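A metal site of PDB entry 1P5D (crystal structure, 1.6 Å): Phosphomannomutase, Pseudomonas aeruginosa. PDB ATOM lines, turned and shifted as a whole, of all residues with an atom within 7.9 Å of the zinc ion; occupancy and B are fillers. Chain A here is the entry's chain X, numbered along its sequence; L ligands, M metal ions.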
ATOM      1  N   ARG A  20      -0.915 -34.187   7.874  1.00  0.00           N
ATOM      2  CA  ARG A  20       0.264 -33.484   8.346  1.00  0.00           C
ATOM      3  C   ARG A  20       1.108 -34.390   9.209  1.00  0.00           C
ATOM      4  O   ARG A  20       0.593 -35.188  10.013  1.00  0.00           O
ATOM      5  CB  ARG A  20      -0.101 -32.217   9.123  1.00  0.00           C
ATOM      6  CG  ARG A  20       1.110 -31.384   9.622  1.00  0.00           C
ATOM      7  CD  ARG A  20       1.244 -30.002   9.012  1.00  0.00           C
ATOM      8  NE  ARG A  20      -0.033 -29.285   9.125  1.00  0.00           N
ATOM      9  CZ  ARG A  20      -0.602 -28.543   8.181  1.00  0.00           C
ATOM     10  NH1 ARG A  20      -0.044 -28.383   6.985  1.00  0.00           N
ATOM     11  NH2 ARG A  20      -1.762 -27.963   8.428  1.00  0.00           N
ATOM     12  N   THR A  87      -0.697 -21.450  -0.563  1.00  0.00           N
ATOM     13  CA  THR A  87      -1.875 -22.278  -0.542  1.00  0.00           C
ATOM     14  C   THR A  87      -3.073 -21.718  -1.321  1.00  0.00           C
ATOM     15  O   THR A  87      -3.628 -22.434  -2.158  1.00  0.00           O
ATOM     16  CB  THR A  87      -2.235 -22.565   0.906  1.00  0.00           C
ATOM     17  OG1 THR A  87      -1.256 -23.454   1.454  1.00  0.00           O
ATOM     18  CG2 THR A  87      -3.609 -23.285   1.031  1.00  0.00           C
ATOM     19  N   PRO A  88      -3.494 -20.465  -1.093  1.00  0.00           N
ATOM     20  CA  PRO A  88      -4.637 -19.960  -1.867  1.00  0.00           C
ATOM     21  C   PRO A  88      -4.414 -19.916  -3.381  1.00  0.00           C
ATOM     22  O   PRO A  88      -5.386 -19.945  -4.138  1.00  0.00           O
ATOM     23  CB  PRO A  88      -4.838 -18.547  -1.327  1.00  0.00           C
ATOM     24  CG  PRO A  88      -3.604 -18.175  -0.691  1.00  0.00           C
ATOM     25  CD  PRO A  88      -3.026 -19.471  -0.089  1.00  0.00           C
ATOM     26  N   TYR A  91      -5.344 -23.255  -4.518  1.00  0.00           N
ATOM     27  CA  TYR A  91      -6.800 -23.290  -4.575  1.00  0.00           C
ATOM     28  C   TYR A  91      -7.347 -22.531  -5.797  1.00  0.00           C
ATOM     29  O   TYR A  91      -8.301 -22.958  -6.430  1.00  0.00           O
ATOM     30  CB  TYR A  91      -7.394 -22.715  -3.298  1.00  0.00           C
ATOM     31  CG  TYR A  91      -7.090 -23.427  -2.003  1.00  0.00           C
ATOM     32  CD1 TYR A  91      -6.758 -24.776  -1.948  1.00  0.00           C
ATOM     33  CD2 TYR A  91      -7.182 -22.749  -0.795  1.00  0.00           C
ATOM     34  CE1 TYR A  91      -6.541 -25.414  -0.746  1.00  0.00           C
ATOM     35  CE2 TYR A  91      -6.956 -23.384   0.405  1.00  0.00           C
ATOM     36  CZ  TYR A  91      -6.639 -24.707   0.430  1.00  0.00           C
ATOM     37  OH  TYR A  91      -6.414 -25.330   1.650  1.00  0.00           O
ATOM     38  N   THR A 106       2.042 -28.631   2.046  1.00  0.00           N
ATOM     39  CA  THR A 106       2.392 -27.596   3.014  1.00  0.00           C
ATOM     40  C   THR A 106       2.344 -28.118   4.441  1.00  0.00           C
ATOM     41  O   THR A 106       1.530 -29.000   4.766  1.00  0.00           O
ATOM     42  CB  THR A 106       1.470 -26.362   2.862  1.00  0.00           C
ATOM     43  OG1 THR A 106       1.842 -25.341   3.808  1.00  0.00           O
ATOM     44  CG2 THR A 106       0.011 -26.707   3.189  1.00  0.00           C
ATOM     45  N   GLY A 107       3.219 -27.538   5.269  1.00  0.00           N
ATOM     46  CA  GLY A 107       3.218 -27.691   6.706  1.00  0.00           C
ATOM     47  C   GLY A 107       2.612 -26.493   7.441  1.00  0.00           C
ATOM     48  O   GLY A 107       2.761 -26.345   8.645  1.00  0.00           O
ATOM     49  N   SEP A 108       1.968 -25.607   6.691  1.00  0.00           N
ATOM     50  CA  SEP A 108       1.205 -24.502   7.252  1.00  0.00           C
ATOM     51  CB  SEP A 108      -0.019 -25.012   8.021  1.00  0.00           C
ATOM     52  OG  SEP A 108      -0.735 -23.900   8.493  1.00  0.00           O
ATOM     53  C   SEP A 108       2.097 -23.542   8.065  1.00  0.00           C
ATOM     54  O   SEP A 108       3.013 -22.955   7.499  1.00  0.00           O
ATOM     55  P   SEP A 108      -2.335 -23.978   8.642  1.00  0.00           P
ATOM     56  O1P SEP A 108      -2.497 -23.870  10.219  1.00  0.00           O
ATOM     57  O2P SEP A 108      -3.002 -25.259   7.999  1.00  0.00           O
ATOM     58  O3P SEP A 108      -2.894 -22.708   7.908  1.00  0.00           O
ATOM     59  N   HIS A 109       1.856 -23.400   9.378  1.00  0.00           N
ATOM     60  CA  HIS A 109       2.616 -22.500  10.233  1.00  0.00           C
ATOM     61  C   HIS A 109       3.570 -23.258  11.182  1.00  0.00           C
ATOM     62  O   HIS A 109       4.182 -22.670  12.069  1.00  0.00           O
ATOM     63  CB  HIS A 109       1.665 -21.657  11.081  1.00  0.00           C
ATOM     64  CG  HIS A 109       0.928 -22.451  12.119  1.00  0.00           C
ATOM     65  ND1 HIS A 109      -0.381 -22.871  11.953  1.00  0.00           N
ATOM     66  CD2 HIS A 109       1.328 -22.946  13.316  1.00  0.00           C
ATOM     67  CE1 HIS A 109      -0.759 -23.573  13.013  1.00  0.00           C
ATOM     68  NE2 HIS A 109       0.260 -23.633  13.849  1.00  0.00           N
ATOM     69  N   ASN A 110       3.656 -24.573  11.007  1.00  0.00           N
ATOM     70  CA  ASN A 110       4.435 -25.439  11.898  1.00  0.00           C
ATOM     71  C   ASN A 110       5.951 -25.275  11.695  1.00  0.00           C
ATOM     72  O   ASN A 110       6.412 -24.670  10.719  1.00  0.00           O
ATOM     73  CB  ASN A 110       4.006 -26.905  11.737  1.00  0.00           C
ATOM     74  CG  ASN A 110       2.614 -27.180  12.293  1.00  0.00           C
ATOM     75  OD1 ASN A 110       1.793 -27.845  11.654  1.00  0.00           O
ATOM     76  ND2 ASN A 110       2.337 -26.679  13.487  1.00  0.00           N
ATOM     77  N   LYS A 118      -3.010 -30.524   1.801  1.00  0.00           N
ATOM     78  CA  LYS A 118      -4.382 -29.982   1.798  1.00  0.00           C
ATOM     79  C   LYS A 118      -4.972 -30.351   0.439  1.00  0.00           C
ATOM     80  O   LYS A 118      -4.332 -30.159  -0.588  1.00  0.00           O
ATOM     81  CB  LYS A 118      -4.366 -28.468   2.057  1.00  0.00           C
ATOM     82  CG  LYS A 118      -3.879 -28.127   3.443  1.00  0.00           C
ATOM     83  CD  LYS A 118      -3.716 -26.643   3.673  1.00  0.00           C
ATOM     84  CE  LYS A 118      -3.327 -26.371   5.097  1.00  0.00           C
ATOM     85  NZ  LYS A 118      -3.371 -24.922   5.430  1.00  0.00           N
ATOM     86  N   PRO A 215       6.137 -18.273  11.330  1.00  0.00           N
ATOM     87  CA  PRO A 215       5.113 -17.551  10.595  1.00  0.00           C
ATOM     88  C   PRO A 215       3.720 -17.998  11.081  1.00  0.00           C
ATOM     89  O   PRO A 215       3.010 -18.750  10.401  1.00  0.00           O
ATOM     90  CB  PRO A 215       5.389 -17.937   9.140  1.00  0.00           C
ATOM     91  CG  PRO A 215       5.941 -19.310   9.225  1.00  0.00           C
ATOM     92  CD  PRO A 215       6.597 -19.461  10.585  1.00  0.00           C
ATOM     93  N   PRO A 217       0.816 -15.759  12.748  1.00  0.00           N
ATOM     94  CA  PRO A 217       0.311 -14.450  13.178  1.00  0.00           C
ATOM     95  C   PRO A 217      -0.789 -14.494  14.244  1.00  0.00           C
ATOM     96  O   PRO A 217      -1.228 -13.439  14.689  1.00  0.00           O
ATOM     97  CB  PRO A 217      -0.246 -13.845  11.876  1.00  0.00           C
ATOM     98  CG  PRO A 217      -0.565 -14.996  11.021  1.00  0.00           C
ATOM     99  CD  PRO A 217       0.415 -16.067  11.368  1.00  0.00           C
ATOM    100  N   PHE A 241       1.405 -12.629   7.548  1.00  0.00           N
ATOM    101  CA  PHE A 241       0.897 -13.850   6.949  1.00  0.00           C
ATOM    102  C   PHE A 241       1.482 -15.078   7.616  1.00  0.00           C
ATOM    103  O   PHE A 241       2.612 -15.067   8.118  1.00  0.00           O
ATOM    104  CB  PHE A 241       1.188 -13.856   5.468  1.00  0.00           C
ATOM    105  CG  PHE A 241       0.550 -12.721   4.733  1.00  0.00           C
ATOM    106  CD1 PHE A 241      -0.815 -12.702   4.507  1.00  0.00           C
ATOM    107  CD2 PHE A 241       1.293 -11.621   4.344  1.00  0.00           C
ATOM    108  CE1 PHE A 241      -1.431 -11.645   3.855  1.00  0.00           C
ATOM    109  CE2 PHE A 241       0.685 -10.572   3.721  1.00  0.00           C
ATOM    110  CZ  PHE A 241      -0.687 -10.566   3.487  1.00  0.00           C
ATOM    111  N   ASP A 242       0.725 -16.175   7.613  1.00  0.00           N
ATOM    112  CA  ASP A 242       1.290 -17.424   8.052  1.00  0.00           C
ATOM    113  C   ASP A 242       2.132 -18.054   6.964  1.00  0.00           C
ATOM    114  O   ASP A 242       2.266 -17.497   5.867  1.00  0.00           O
ATOM    115  CB  ASP A 242       0.244 -18.381   8.629  1.00  0.00           C
ATOM    116  CG  ASP A 242      -0.519 -19.144   7.603  1.00  0.00           C
ATOM    117  OD1 ASP A 242      -0.700 -18.664   6.456  1.00  0.00           O
ATOM    118  OD2 ASP A 242      -1.051 -20.240   7.910  1.00  0.00           O
ATOM    119  N   GLY A 243       2.729 -19.184   7.279  1.00  0.00           N
ATOM    120  CA  GLY A 243       3.750 -19.756   6.425  1.00  0.00           C
ATOM    121  C   GLY A 243       3.285 -20.046   5.023  1.00  0.00           C
ATOM    122  O   GLY A 243       4.067 -19.939   4.071  1.00  0.00           O
ATOM    123  N   ASP A 244       2.010 -20.388   4.846  1.00  0.00           N
ATOM    124  CA  ASP A 244       1.496 -20.771   3.528  1.00  0.00           C
ATOM    125  C   ASP A 244       0.533 -19.748   2.918  1.00  0.00           C
ATOM    126  O   ASP A 244       0.038 -19.962   1.830  1.00  0.00           O
ATOM    127  CB  ASP A 244       0.918 -22.207   3.509  1.00  0.00           C
ATOM    128  CG  ASP A 244      -0.292 -22.390   4.386  1.00  0.00           C
ATOM    129  OD1 ASP A 244      -0.311 -21.782   5.486  1.00  0.00           O
ATOM    130  OD2 ASP A 244      -1.215 -23.188   4.126  1.00  0.00           O
ATOM    131  N   GLY A 245       0.284 -18.630   3.605  1.00  0.00           N
ATOM    132  CA  GLY A 245      -0.507 -17.542   3.078  1.00  0.00           C
ATOM    133  C   GLY A 245      -2.016 -17.640   3.144  1.00  0.00           C
ATOM    134  O   GLY A 245      -2.698 -16.821   2.536  1.00  0.00           O
ATOM    135  N   ASP A 246      -2.547 -18.637   3.860  1.00  0.00           N
ATOM    136  CA  ASP A 246      -4.001 -18.745   3.980  1.00  0.00           C
ATOM    137  C   ASP A 246      -4.533 -18.105   5.254  1.00  0.00           C
ATOM    138  O   ASP A 246      -5.746 -18.069   5.451  1.00  0.00           O
ATOM    139  CB  ASP A 246      -4.525 -20.183   3.831  1.00  0.00           C
ATOM    140  CG  ASP A 246      -3.948 -21.124   4.827  1.00  0.00           C
ATOM    141  OD1 ASP A 246      -3.163 -20.685   5.707  1.00  0.00           O
ATOM    142  OD2 ASP A 246      -4.186 -22.347   4.795  1.00  0.00           O
ATOM    143  N   ARG A 247      -3.638 -17.624   6.106  1.00  0.00           N
ATOM    144  CA  ARG A 247      -3.992 -16.852   7.315  1.00  0.00           C
ATOM    145  C   ARG A 247      -3.465 -15.437   7.181  1.00  0.00           C
ATOM    146  O   ARG A 247      -2.458 -15.200   6.502  1.00  0.00           O
ATOM    147  CB  ARG A 247      -3.388 -17.451   8.590  1.00  0.00           C
ATOM    148  CG  ARG A 247      -3.832 -18.855   8.984  1.00  0.00           C
ATOM    149  CD  ARG A 247      -3.145 -19.391  10.253  1.00  0.00           C
ATOM    150  NE  ARG A 247      -3.678 -20.700  10.654  1.00  0.00           N
ATOM    151  CZ  ARG A 247      -3.592 -21.205  11.888  1.00  0.00           C
ATOM    152  NH1 ARG A 247      -2.985 -20.533  12.871  1.00  0.00           N
ATOM    153  NH2 ARG A 247      -4.108 -22.392  12.148  1.00  0.00           N
ATOM    154  N   VAL A 248      -4.127 -14.496   7.849  1.00  0.00           N
ATOM    155  CA  VAL A 248      -3.627 -13.132   7.945  1.00  0.00           C
ATOM    156  C   VAL A 248      -3.832 -12.634   9.362  1.00  0.00           C
ATOM    157  O   VAL A 248      -4.771 -13.048  10.052  1.00  0.00           O
ATOM    158  CB  VAL A 248      -4.341 -12.210   6.930  1.00  0.00           C
ATOM    159  CG1 VAL A 248      -5.851 -12.114   7.167  1.00  0.00           C
ATOM    160  CG2 VAL A 248      -3.663 -10.854   6.849  1.00  0.00           C
ATOM    161  N   HIS A 308     -10.522 -25.212   8.657  1.00  0.00           N
ATOM    162  CA  HIS A 308     -10.652 -24.595   7.352  1.00  0.00           C
ATOM    163  C   HIS A 308     -11.463 -25.462   6.391  1.00  0.00           C
ATOM    164  O   HIS A 308     -12.359 -24.959   5.732  1.00  0.00           O
ATOM    165  CB  HIS A 308      -9.291 -24.246   6.776  1.00  0.00           C
ATOM    166  CG  HIS A 308      -8.471 -25.425   6.384  1.00  0.00           C
ATOM    167  ND1 HIS A 308      -8.297 -25.795   5.064  1.00  0.00           N
ATOM    168  CD2 HIS A 308      -7.796 -26.342   7.120  1.00  0.00           C
ATOM    169  CE1 HIS A 308      -7.508 -26.855   5.013  1.00  0.00           C
ATOM    170  NE2 HIS A 308      -7.188 -27.208   6.243  1.00  0.00           N
ATOM    171  N   HIS A 329      -8.077 -17.557   9.023  1.00  0.00           N
ATOM    172  CA  HIS A 329      -8.538 -18.038   7.733  1.00  0.00           C
ATOM    173  C   HIS A 329      -9.810 -17.258   7.386  1.00  0.00           C
ATOM    174  O   HIS A 329     -10.795 -17.325   8.123  1.00  0.00           O
ATOM    175  CB  HIS A 329      -8.888 -19.559   7.726  1.00  0.00           C
ATOM    176  CG  HIS A 329      -7.722 -20.486   7.955  1.00  0.00           C
ATOM    177  ND1 HIS A 329      -6.886 -20.893   6.946  1.00  0.00           N
ATOM    178  CD2 HIS A 329      -7.365 -21.200   9.050  1.00  0.00           C
ATOM    179  CE1 HIS A 329      -5.957 -21.705   7.436  1.00  0.00           C
ATOM    180  NE2 HIS A 329      -6.223 -21.915   8.714  1.00  0.00           N
ATOM    181  N   ASP A 340     -10.217 -19.924   1.524  1.00  0.00           N
ATOM    182  CA  ASP A 340      -9.426 -19.108   2.441  1.00  0.00           C
ATOM    183  C   ASP A 340      -8.147 -18.577   1.785  1.00  0.00           C
ATOM    184  O   ASP A 340      -7.443 -19.300   1.087  1.00  0.00           O
ATOM    185  CB  ASP A 340      -9.102 -19.801   3.772  1.00  0.00           C
ATOM    186  CG  ASP A 340      -8.630 -21.238   3.629  1.00  0.00           C
ATOM    187  OD1 ASP A 340      -9.154 -21.985   2.780  1.00  0.00           O
ATOM    188  OD2 ASP A 340      -7.772 -21.690   4.432  1.00  0.00           O
HETATM  189  C1  LIG L   1      -6.654 -24.781  14.036  1.00  0.00           C
HETATM  190  C2  LIG L   1      -7.438 -23.485  13.940  1.00  0.00           C
HETATM  191  C3  LIG L   1      -8.441 -23.528  12.784  1.00  0.00           C
HETATM  192  C4  LIG L   1      -7.671 -23.694  11.476  1.00  0.00           C
HETATM  193  C5  LIG L   1      -6.758 -24.921  11.528  1.00  0.00           C
HETATM  194  C6  LIG L   1      -5.803 -24.996  10.299  1.00  0.00           C
HETATM  195  O1  LIG L   1      -7.538 -25.872  14.253  1.00  0.00           O
HETATM  196  O2  LIG L   1      -8.131 -23.204  15.190  1.00  0.00           O
HETATM  197  O3  LIG L   1      -9.174 -22.308  12.756  1.00  0.00           O
HETATM  198  O4  LIG L   1      -8.574 -23.880  10.395  1.00  0.00           O
HETATM  199  O5  LIG L   1      -5.947 -24.993  12.760  1.00  0.00           O
HETATM  200  O6  LIG L   1      -5.142 -23.753  10.439  1.00  0.00           O
HETATM  201  P1  LIG L   1      -7.695 -26.585  15.697  1.00  0.00           P
HETATM  202  O7  LIG L   1      -8.355 -25.567  16.603  1.00  0.00           O
HETATM  203  O8  LIG L   1      -6.356 -27.007  16.215  1.00  0.00           O
HETATM  204  O9  LIG L   1      -8.615 -27.713  15.426  1.00  0.00           O
HETATM  205 ZN    ZN M   1      -1.843 -21.560   6.761  1.00  0.00          ZN
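O1P of SEP 108 sits at hydrogen-bond distance from an oxygen (O6) of the ligand (2.7 Å). The guanidinium group (NH2) of Arg 247 sits at hydrogen-bond distance from an oxygen (O6) of the ligand, at 2.4 Å. An oxygen (O6) of the ligand lies within hydrogen-bond range of a ring nitrogen (NE2) of His 329 (2.7 Å). The backbone NH of His 308 is in hydrogen-bond range of an oxygen (O4) of the ligand (2.9 Å).
OD1 of Asp 246 binds the zinc ion (1.9 Å). The zinc ion is bound by OD2 of Asp 242, at 1.9 Å. O3P of SEP 108 binds the zinc ion, 1.9 Å away. The zinc ion is bound by OD1 of Asp 244. The zinc ion has four donor atoms within binding distance.
OD2 of Asp 246 lies within salt-bridge range of NZ of Lys 118 (2.8 Å). The backbone carbonyl oxygen (O) of Asp 246 sits at hydrogen-bond distance from a ring nitrogen (ND1) of His 329 (3.4 Å). OD1 of Asp 242 lies within hydrogen-bond range of N of Gly 245. O2P of SEP 108 is in salt-bridge range of NZ of Lys 118 (2.6 Å). O1P of SEP 108 lies within salt-bridge range of the guanidinium group (NH2) of Arg 247, at 2.9 Å. A ring nitrogen (ND1) of His 109 sits at hydrogen-bond distance from O1P of SEP 108 (2.9 Å). N of SEP 108 is in hydrogen-bond range of the side-chain hydroxyl (OG1) of Thr 106, at 2.9 Å. The side-chain carboxylate of Asp 244 is in hydrogen-bond range of the side-chain hydroxyl of Thr 87 (2.7 Å).
Lys 118 touches the zinc ion (NZ to ZN, 3.9 Å). Five residues have an atom within 4 Å of the zinc ion: SEP 108, Lys 118, Asp 242, Asp 244 and Asp 246. Along chain A the residues within 4 Å of the zinc ion span positions 108 to 246.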
